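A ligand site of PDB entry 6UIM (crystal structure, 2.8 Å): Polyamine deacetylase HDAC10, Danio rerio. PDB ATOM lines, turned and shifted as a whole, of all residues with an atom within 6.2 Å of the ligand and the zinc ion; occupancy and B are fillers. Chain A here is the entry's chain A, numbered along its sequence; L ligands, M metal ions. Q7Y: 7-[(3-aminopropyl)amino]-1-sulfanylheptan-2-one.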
ATOM      1  N   ALA A  24     -12.546   9.430 -30.728  1.00  0.00           N
ATOM      2  CA  ALA A  24     -12.129   8.408 -29.777  1.00  0.00           C
ATOM      3  C   ALA A  24     -12.141   7.018 -30.405  1.00  0.00           C
ATOM      4  O   ALA A  24     -11.354   6.157 -30.001  1.00  0.00           O
ATOM      5  CB  ALA A  24     -13.049   8.439 -28.549  1.00  0.00           C
ATOM      6  N   CYS A  25     -13.012   6.800 -31.401  1.00  0.00           N
ATOM      7  CA  CYS A  25     -13.239   5.485 -31.988  1.00  0.00           C
ATOM      8  C   CYS A  25     -12.597   5.330 -33.355  1.00  0.00           C
ATOM      9  O   CYS A  25     -12.579   4.217 -33.901  1.00  0.00           O
ATOM     10  CB  CYS A  25     -14.754   5.249 -32.116  1.00  0.00           C
ATOM     11  SG  CYS A  25     -15.649   5.107 -30.555  1.00  0.00           S
ATOM     12  N   ILE A  27      -9.711   5.081 -34.400  1.00  0.00           N
ATOM     13  CA  ILE A  27      -8.592   4.162 -34.539  1.00  0.00           C
ATOM     14  C   ILE A  27      -9.044   2.733 -34.737  1.00  0.00           C
ATOM     15  O   ILE A  27      -8.287   1.914 -35.286  1.00  0.00           O
ATOM     16  CB  ILE A  27      -7.659   4.254 -33.313  1.00  0.00           C
ATOM     17  CG1 ILE A  27      -8.426   3.905 -32.032  1.00  0.00           C
ATOM     18  CG2 ILE A  27      -7.047   5.641 -33.222  1.00  0.00           C
ATOM     19  CD1 ILE A  27      -7.542   3.746 -30.817  1.00  0.00           C
ATOM     20  N   ASP A  94     -17.196   5.372 -25.257  1.00  0.00           N
ATOM     21  CA  ASP A  94     -16.162   5.062 -26.247  1.00  0.00           C
ATOM     22  C   ASP A  94     -16.463   3.768 -27.000  1.00  0.00           C
ATOM     23  O   ASP A  94     -15.609   2.887 -27.130  1.00  0.00           O
ATOM     24  CB  ASP A  94     -14.788   4.993 -25.581  1.00  0.00           C
ATOM     25  CG  ASP A  94     -14.218   6.359 -25.309  1.00  0.00           C
ATOM     26  OD1 ASP A  94     -14.793   7.357 -25.806  1.00  0.00           O
ATOM     27  OD2 ASP A  94     -13.180   6.436 -24.601  1.00  0.00           O
ATOM     28  N   PRO A 134     -13.167  -6.254 -29.893  1.00  0.00           N
ATOM     29  CA  PRO A 134     -12.482  -6.840 -28.727  1.00  0.00           C
ATOM     30  C   PRO A 134     -13.459  -7.110 -27.601  1.00  0.00           C
ATOM     31  O   PRO A 134     -14.673  -7.043 -27.802  1.00  0.00           O
ATOM     32  CB  PRO A 134     -11.462  -5.757 -28.332  1.00  0.00           C
ATOM     33  CG  PRO A 134     -11.449  -4.773 -29.478  1.00  0.00           C
ATOM     34  CD  PRO A 134     -12.802  -4.843 -30.070  1.00  0.00           C
ATOM     35  N   HIS A 136     -12.302  -7.170 -23.552  1.00  0.00           N
ATOM     36  CA  HIS A 136     -11.963  -7.057 -22.139  1.00  0.00           C
ATOM     37  C   HIS A 136     -12.534  -5.825 -21.449  1.00  0.00           C
ATOM     38  O   HIS A 136     -12.447  -5.729 -20.225  1.00  0.00           O
ATOM     39  CB  HIS A 136     -10.439  -7.104 -21.947  1.00  0.00           C
ATOM     40  CG  HIS A 136      -9.701  -5.959 -22.575  1.00  0.00           C
ATOM     41  ND1 HIS A 136      -8.354  -5.742 -22.357  1.00  0.00           N
ATOM     42  CD2 HIS A 136     -10.105  -4.988 -23.410  1.00  0.00           C
ATOM     43  CE1 HIS A 136      -7.965  -4.683 -23.044  1.00  0.00           C
ATOM     44  NE2 HIS A 136      -9.018  -4.197 -23.688  1.00  0.00           N
ATOM     45  N   HIS A 137     -13.144  -4.889 -22.188  1.00  0.00           N
ATOM     46  CA  HIS A 137     -13.761  -3.744 -21.540  1.00  0.00           C
ATOM     47  C   HIS A 137     -15.267  -3.903 -21.351  1.00  0.00           C
ATOM     48  O   HIS A 137     -15.844  -3.170 -20.537  1.00  0.00           O
ATOM     49  CB  HIS A 137     -13.494  -2.471 -22.351  1.00  0.00           C
ATOM     50  CG  HIS A 137     -12.064  -2.083 -22.391  1.00  0.00           C
ATOM     51  ND1 HIS A 137     -11.311  -1.908 -21.247  1.00  0.00           N
ATOM     52  CD2 HIS A 137     -11.217  -1.866 -23.428  1.00  0.00           C
ATOM     53  CE1 HIS A 137     -10.072  -1.577 -21.585  1.00  0.00           C
ATOM     54  NE2 HIS A 137      -9.995  -1.553 -22.893  1.00  0.00           N
ATOM     55  N   GLY A 145     -15.625   0.812 -24.436  1.00  0.00           N
ATOM     56  CA  GLY A 145     -14.331   0.883 -25.064  1.00  0.00           C
ATOM     57  C   GLY A 145     -14.105  -0.084 -26.210  1.00  0.00           C
ATOM     58  O   GLY A 145     -13.247  -0.958 -26.116  1.00  0.00           O
ATOM     59  N   PHE A 146     -14.897   0.067 -27.289  1.00  0.00           N
ATOM     60  CA  PHE A 146     -14.772  -0.682 -28.535  1.00  0.00           C
ATOM     61  C   PHE A 146     -15.325  -2.102 -28.444  1.00  0.00           C
ATOM     62  O   PHE A 146     -15.487  -2.770 -29.479  1.00  0.00           O
ATOM     63  CB  PHE A 146     -13.311  -0.759 -29.008  1.00  0.00           C
ATOM     64  CG  PHE A 146     -12.652   0.580 -29.246  1.00  0.00           C
ATOM     65  CD1 PHE A 146     -13.388   1.758 -29.319  1.00  0.00           C
ATOM     66  CD2 PHE A 146     -11.281   0.646 -29.430  1.00  0.00           C
ATOM     67  CE1 PHE A 146     -12.759   2.969 -29.549  1.00  0.00           C
ATOM     68  CE2 PHE A 146     -10.647   1.859 -29.673  1.00  0.00           C
ATOM     69  CZ  PHE A 146     -11.385   3.016 -29.733  1.00  0.00           C
ATOM     70  N   CYS A 147     -15.616  -2.575 -27.231  1.00  0.00           N
ATOM     71  CA  CYS A 147     -16.000  -3.960 -26.984  1.00  0.00           C
ATOM     72  C   CYS A 147     -17.497  -4.099 -26.713  1.00  0.00           C
ATOM     73  O   CYS A 147     -18.068  -3.334 -25.924  1.00  0.00           O
ATOM     74  CB  CYS A 147     -15.217  -4.540 -25.814  1.00  0.00           C
ATOM     75  SG  CYS A 147     -13.500  -4.027 -25.718  1.00  0.00           S
ATOM     76  N   ASP A 174      -2.706  -5.957 -23.155  1.00  0.00           N
ATOM     77  CA  ASP A 174      -3.162  -4.675 -23.671  1.00  0.00           C
ATOM     78  C   ASP A 174      -2.755  -3.550 -22.705  1.00  0.00           C
ATOM     79  O   ASP A 174      -2.476  -3.777 -21.521  1.00  0.00           O
ATOM     80  CB  ASP A 174      -4.685  -4.729 -23.848  1.00  0.00           C
ATOM     81  CG  ASP A 174      -5.195  -3.702 -24.838  1.00  0.00           C
ATOM     82  OD1 ASP A 174      -4.976  -2.494 -24.631  1.00  0.00           O
ATOM     83  OD2 ASP A 174      -5.833  -4.125 -25.832  1.00  0.00           O
ATOM     84  N   VAL A 175      -2.683  -2.323 -23.239  1.00  0.00           N
ATOM     85  CA  VAL A 175      -2.360  -1.138 -22.424  1.00  0.00           C
ATOM     86  C   VAL A 175      -3.563  -0.557 -21.704  1.00  0.00           C
ATOM     87  O   VAL A 175      -3.416   0.417 -20.948  1.00  0.00           O
ATOM     88  CB  VAL A 175      -1.747   0.039 -23.209  1.00  0.00           C
ATOM     89  CG1 VAL A 175      -0.247  -0.157 -23.399  1.00  0.00           C
ATOM     90  CG2 VAL A 175      -2.457   0.208 -24.528  1.00  0.00           C
ATOM     91  N   HIS A 176      -4.755  -1.084 -21.938  1.00  0.00           N
ATOM     92  CA  HIS A 176      -5.954  -0.653 -21.244  1.00  0.00           C
ATOM     93  C   HIS A 176      -6.346  -1.708 -20.221  1.00  0.00           C
ATOM     94  O   HIS A 176      -6.200  -2.906 -20.468  1.00  0.00           O
ATOM     95  CB  HIS A 176      -7.087  -0.407 -22.232  1.00  0.00           C
ATOM     96  CG  HIS A 176      -6.789   0.632 -23.249  1.00  0.00           C
ATOM     97  ND1 HIS A 176      -6.136   0.353 -24.431  1.00  0.00           N
ATOM     98  CD2 HIS A 176      -7.045   1.958 -23.266  1.00  0.00           C
ATOM     99  CE1 HIS A 176      -6.006   1.470 -25.134  1.00  0.00           C
ATOM    100  NE2 HIS A 176      -6.549   2.454 -24.454  1.00  0.00           N
ATOM    101  N   ARG A 198      -1.695   1.166 -19.114  1.00  0.00           N
ATOM    102  CA  ARG A 198      -1.335   2.570 -18.964  1.00  0.00           C
ATOM    103  C   ARG A 198      -2.298   3.237 -17.999  1.00  0.00           C
ATOM    104  O   ARG A 198      -3.519   3.223 -18.225  1.00  0.00           O
ATOM    105  CB  ARG A 198      -1.325   3.273 -20.311  1.00  0.00           C
ATOM    106  CG  ARG A 198      -0.980   4.748 -20.245  1.00  0.00           C
ATOM    107  CD  ARG A 198      -1.072   5.394 -21.623  1.00  0.00           C
ATOM    108  NE  ARG A 198      -0.955   6.851 -21.560  1.00  0.00           N
ATOM    109  CZ  ARG A 198      -1.102   7.656 -22.611  1.00  0.00           C
ATOM    110  NH1 ARG A 198      -1.380   7.153 -23.802  1.00  0.00           N
ATOM    111  NH2 ARG A 198      -0.969   8.972 -22.461  1.00  0.00           N
ATOM    112  N   PHE A 204      -5.536   8.388 -17.155  1.00  0.00           N
ATOM    113  CA  PHE A 204      -5.700   7.764 -18.462  1.00  0.00           C
ATOM    114  C   PHE A 204      -6.926   6.854 -18.490  1.00  0.00           C
ATOM    115  O   PHE A 204      -7.324   6.285 -17.467  1.00  0.00           O
ATOM    116  CB  PHE A 204      -4.465   6.950 -18.860  1.00  0.00           C
ATOM    117  CG  PHE A 204      -4.470   6.507 -20.294  1.00  0.00           C
ATOM    118  CD1 PHE A 204      -4.386   7.440 -21.316  1.00  0.00           C
ATOM    119  CD2 PHE A 204      -4.582   5.166 -20.614  1.00  0.00           C
ATOM    120  CE1 PHE A 204      -4.397   7.034 -22.643  1.00  0.00           C
ATOM    121  CE2 PHE A 204      -4.601   4.749 -21.937  1.00  0.00           C
ATOM    122  CZ  PHE A 204      -4.505   5.694 -22.953  1.00  0.00           C
ATOM    123  N   TRP A 205      -7.512   6.737 -19.683  1.00  0.00           N
ATOM    124  CA  TRP A 205      -8.732   5.973 -19.872  1.00  0.00           C
ATOM    125  C   TRP A 205      -8.508   4.503 -19.489  1.00  0.00           C
ATOM    126  O   TRP A 205      -7.481   3.917 -19.846  1.00  0.00           O
ATOM    127  CB  TRP A 205      -9.196   6.062 -21.320  1.00  0.00           C
ATOM    128  CG  TRP A 205     -10.573   5.556 -21.544  1.00  0.00           C
ATOM    129  CD1 TRP A 205     -11.736   6.277 -21.539  1.00  0.00           C
ATOM    130  CD2 TRP A 205     -10.951   4.191 -21.775  1.00  0.00           C
ATOM    131  NE1 TRP A 205     -12.802   5.447 -21.754  1.00  0.00           N
ATOM    132  CE2 TRP A 205     -12.356   4.165 -21.893  1.00  0.00           C
ATOM    133  CE3 TRP A 205     -10.239   2.992 -21.875  1.00  0.00           C
ATOM    134  CZ2 TRP A 205     -13.055   2.990 -22.133  1.00  0.00           C
ATOM    135  CZ3 TRP A 205     -10.937   1.827 -22.106  1.00  0.00           C
ATOM    136  CH2 TRP A 205     -12.341   1.832 -22.237  1.00  0.00           C
ATOM    137  N   GLY A 265      -3.613  -7.708 -26.740  1.00  0.00           N
ATOM    138  CA  GLY A 265      -3.758  -6.414 -27.373  1.00  0.00           C
ATOM    139  C   GLY A 265      -2.389  -5.849 -27.700  1.00  0.00           C
ATOM    140  O   GLY A 265      -1.523  -5.772 -26.824  1.00  0.00           O
ATOM    141  N   ASP A 267      -1.657  -2.770 -28.866  1.00  0.00           N
ATOM    142  CA  ASP A 267      -1.470  -1.334 -28.668  1.00  0.00           C
ATOM    143  C   ASP A 267      -0.452  -1.033 -27.574  1.00  0.00           C
ATOM    144  O   ASP A 267      -0.216   0.146 -27.286  1.00  0.00           O
ATOM    145  CB  ASP A 267      -2.798  -0.646 -28.335  1.00  0.00           C
ATOM    146  CG  ASP A 267      -3.613  -1.415 -27.316  1.00  0.00           C
ATOM    147  OD1 ASP A 267      -3.109  -2.415 -26.779  1.00  0.00           O
ATOM    148  OD2 ASP A 267      -4.755  -0.999 -27.044  1.00  0.00           O
ATOM    149  N   PRO A 273      -0.897   4.826 -31.427  1.00  0.00           N
ATOM    150  CA  PRO A 273      -1.364   6.173 -31.099  1.00  0.00           C
ATOM    151  C   PRO A 273      -2.101   6.263 -29.776  1.00  0.00           C
ATOM    152  O   PRO A 273      -2.380   7.365 -29.307  1.00  0.00           O
ATOM    153  CB  PRO A 273      -2.295   6.516 -32.272  1.00  0.00           C
ATOM    154  CG  PRO A 273      -2.828   5.189 -32.702  1.00  0.00           C
ATOM    155  CD  PRO A 273      -1.692   4.207 -32.510  1.00  0.00           C
ATOM    156  N   GLU A 274      -2.430   5.125 -29.164  1.00  0.00           N
ATOM    157  CA  GLU A 274      -3.189   5.101 -27.913  1.00  0.00           C
ATOM    158  C   GLU A 274      -2.339   4.734 -26.706  1.00  0.00           C
ATOM    159  O   GLU A 274      -2.519   5.315 -25.635  1.00  0.00           O
ATOM    160  CB  GLU A 274      -4.350   4.111 -28.028  1.00  0.00           C
ATOM    161  CG  GLU A 274      -5.356   4.191 -26.908  1.00  0.00           C
ATOM    162  CD  GLU A 274      -6.417   5.237 -27.156  1.00  0.00           C
ATOM    163  OE1 GLU A 274      -7.078   5.640 -26.182  1.00  0.00           O
ATOM    164  OE2 GLU A 274      -6.575   5.656 -28.312  1.00  0.00           O
ATOM    165  N   GLU A 276       1.201   4.624 -26.597  1.00  0.00           N
ATOM    166  CA  GLU A 276       2.401   5.448 -26.565  1.00  0.00           C
ATOM    167  C   GLU A 276       3.542   4.782 -25.807  1.00  0.00           C
ATOM    168  O   GLU A 276       4.344   5.450 -25.162  1.00  0.00           O
ATOM    169  CB  GLU A 276       2.107   6.830 -25.963  1.00  0.00           C
ATOM    170  CG  GLU A 276       1.082   7.657 -26.744  1.00  0.00           C
ATOM    171  CD  GLU A 276       0.765   8.972 -26.043  1.00  0.00           C
ATOM    172  OE1 GLU A 276       1.352   9.223 -24.976  1.00  0.00           O
ATOM    173  OE2 GLU A 276      -0.076   9.745 -26.560  1.00  0.00           O
ATOM    174  N   GLU A 304      -7.074  -8.411 -28.970  1.00  0.00           N
ATOM    175  CA  GLU A 304      -7.763  -7.371 -28.223  1.00  0.00           C
ATOM    176  C   GLU A 304      -7.616  -6.038 -28.955  1.00  0.00           C
ATOM    177  O   GLU A 304      -8.429  -5.721 -29.829  1.00  0.00           O
ATOM    178  CB  GLU A 304      -7.214  -7.305 -26.796  1.00  0.00           C
ATOM    179  CG  GLU A 304      -8.241  -6.984 -25.734  1.00  0.00           C
ATOM    180  CD  GLU A 304      -9.330  -8.037 -25.594  1.00  0.00           C
ATOM    181  OE1 GLU A 304     -10.453  -7.788 -26.057  1.00  0.00           O
ATOM    182  OE2 GLU A 304      -9.048  -9.115 -25.017  1.00  0.00           O
ATOM    183  N   GLY A 305      -6.579  -5.275 -28.627  1.00  0.00           N
ATOM    184  CA  GLY A 305      -6.322  -3.996 -29.250  1.00  0.00           C
ATOM    185  C   GLY A 305      -5.065  -3.988 -30.097  1.00  0.00           C
ATOM    186  O   GLY A 305      -4.416  -5.013 -30.332  1.00  0.00           O
ATOM    187  N   GLY A 306      -4.707  -2.787 -30.563  1.00  0.00           N
ATOM    188  CA  GLY A 306      -3.599  -2.579 -31.479  1.00  0.00           C
ATOM    189  C   GLY A 306      -4.049  -1.772 -32.676  1.00  0.00           C
ATOM    190  O   GLY A 306      -4.877  -2.239 -33.461  1.00  0.00           O
ATOM    191  N   TYR A 307      -3.527  -0.548 -32.842  1.00  0.00           N
ATOM    192  CA  TYR A 307      -4.100   0.377 -33.812  1.00  0.00           C
ATOM    193  C   TYR A 307      -3.096   1.034 -34.740  1.00  0.00           C
ATOM    194  O   TYR A 307      -3.499   1.893 -35.538  1.00  0.00           O
ATOM    195  CB  TYR A 307      -4.909   1.458 -33.072  1.00  0.00           C
ATOM    196  CG  TYR A 307      -5.898   0.865 -32.109  1.00  0.00           C
ATOM    197  CD1 TYR A 307      -7.174   0.520 -32.524  1.00  0.00           C
ATOM    198  CD2 TYR A 307      -5.538   0.608 -30.795  1.00  0.00           C
ATOM    199  CE1 TYR A 307      -8.081  -0.039 -31.639  1.00  0.00           C
ATOM    200  CE2 TYR A 307      -6.432   0.051 -29.905  1.00  0.00           C
ATOM    201  CZ  TYR A 307      -7.707  -0.263 -30.332  1.00  0.00           C
ATOM    202  OH  TYR A 307      -8.605  -0.820 -29.452  1.00  0.00           O
HETATM  203  C10 Q7Y L   1     -10.318   1.345 -26.009  1.00  0.00           C
HETATM  204  C11 Q7Y L   1      -9.325   0.309 -26.448  1.00  0.00           C
HETATM  205  C13 Q7Y L   1      -9.764  -1.121 -26.457  1.00  0.00           C
HETATM  206  C02 Q7Y L   1      -6.087   8.797 -25.242  1.00  0.00           C
HETATM  207  C03 Q7Y L   1      -7.601   9.076 -25.288  1.00  0.00           C
HETATM  208  C04 Q7Y L   1      -8.370   7.925 -24.603  1.00  0.00           C
HETATM  209  C06 Q7Y L   1      -9.967   6.060 -25.124  1.00  0.00           C
HETATM  210  C07 Q7Y L   1     -10.411   5.217 -26.328  1.00  0.00           C
HETATM  211  C08 Q7Y L   1     -10.848   3.811 -25.927  1.00  0.00           C
HETATM  212  C09 Q7Y L   1      -9.948   2.731 -26.500  1.00  0.00           C
HETATM  213  N01 Q7Y L   1      -5.389   9.647 -26.218  1.00  0.00           N
HETATM  214  N05 Q7Y L   1      -9.262   7.278 -25.591  1.00  0.00           N
HETATM  215  O12 Q7Y L   1      -8.193   0.602 -26.794  1.00  0.00           O
HETATM  216  S14 Q7Y L   1      -8.345  -2.149 -26.183  1.00  0.00           S
HETATM  217 ZN    ZN M   1      -6.318  -1.449 -25.715  1.00  0.00          ZN
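A ring nitrogen (NE2) of His 136 sits close to a sulfur (S14) of the ligand (3.3 Å).
The side-chain hydroxyl (OH) of Tyr 307 sits at hydrogen-bond distance from an oxygen (O12) of the ligand.
NE2 of His 137 sits close to S14 of the ligand (3.7 Å).
A nitrogen (N05) of the ligand is in salt-bridge range of the side-chain carboxylate (OE1) of Glu 274, at 2.8 Å.
A ring nitrogen (NE2) of His 136 sits at hydrogen-bond distance from a ring nitrogen (NE2) of His 137, 2.9 Å away.
N of His 137 is in hydrogen-bond range of SG of Cys 147, 3.7 Å away.
SG of Cys 147 lies within hydrogen-bond range of O of Gly 145, at 3.1 Å.
N of Phe 146 sits at hydrogen-bond distance from O of Asp 94 (2.9 Å).
The backbone carbonyl oxygen of Asp 94 sits close to the backbone NH of Gly 145 (3.4 Å).
NH1 of Arg 198 sits at hydrogen-bond distance from O of Glu 274 (2.8 Å).
OD2 of Asp 94 is in hydrogen-bond range of NE1 of Trp 205 (3.0 Å).
The backbone NH (N) of His 136 is in hydrogen-bond range of the side-chain carboxylate (OE1) of Glu 304 (3.2 Å).
Ala 24 touches the ligand.
OD2 of Asp 94 touches C06 of the ligand, at 3.3 Å.
Gly 145 touches the ligand (O to C13, 3.5 Å).
Phe 146 touches the ligand.
Phe 204 touches the ligand.
Trp 205 touches the ligand.
Hydrophobic or aromatic side chains within 4 Å of the ligand: His 137, Phe 146, His 176, Phe 204, Trp 205 and Tyr 307.
Within 4 Å of the ligand: Ala 24, Asp 94, His 136, His 137, Gly 145, Phe 146, Asp 174, His 176, Phe 204, Trp 205, Asp 267, Glu 274 and Tyr 307.
The nearest printed residue that does not touch the ligand is Gly 305 (4.1 Å).
Of the 25 residues printed, 3 come within 4 Å of the zinc ion.
The zinc ion is bound by the side-chain carboxylate (OD1) of Asp 174 (2.0 Å), the side-chain carboxylate (OD2) of Asp 267 (2.1 Å), a sulfur (S14) of the ligand (2.2 Å) and a ring nitrogen (ND1) of His 176 (2.2 Å).
Slightly farther from the zinc ion lies the side-chain carboxylate (OD2) of Asp 174 (2.7 Å).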
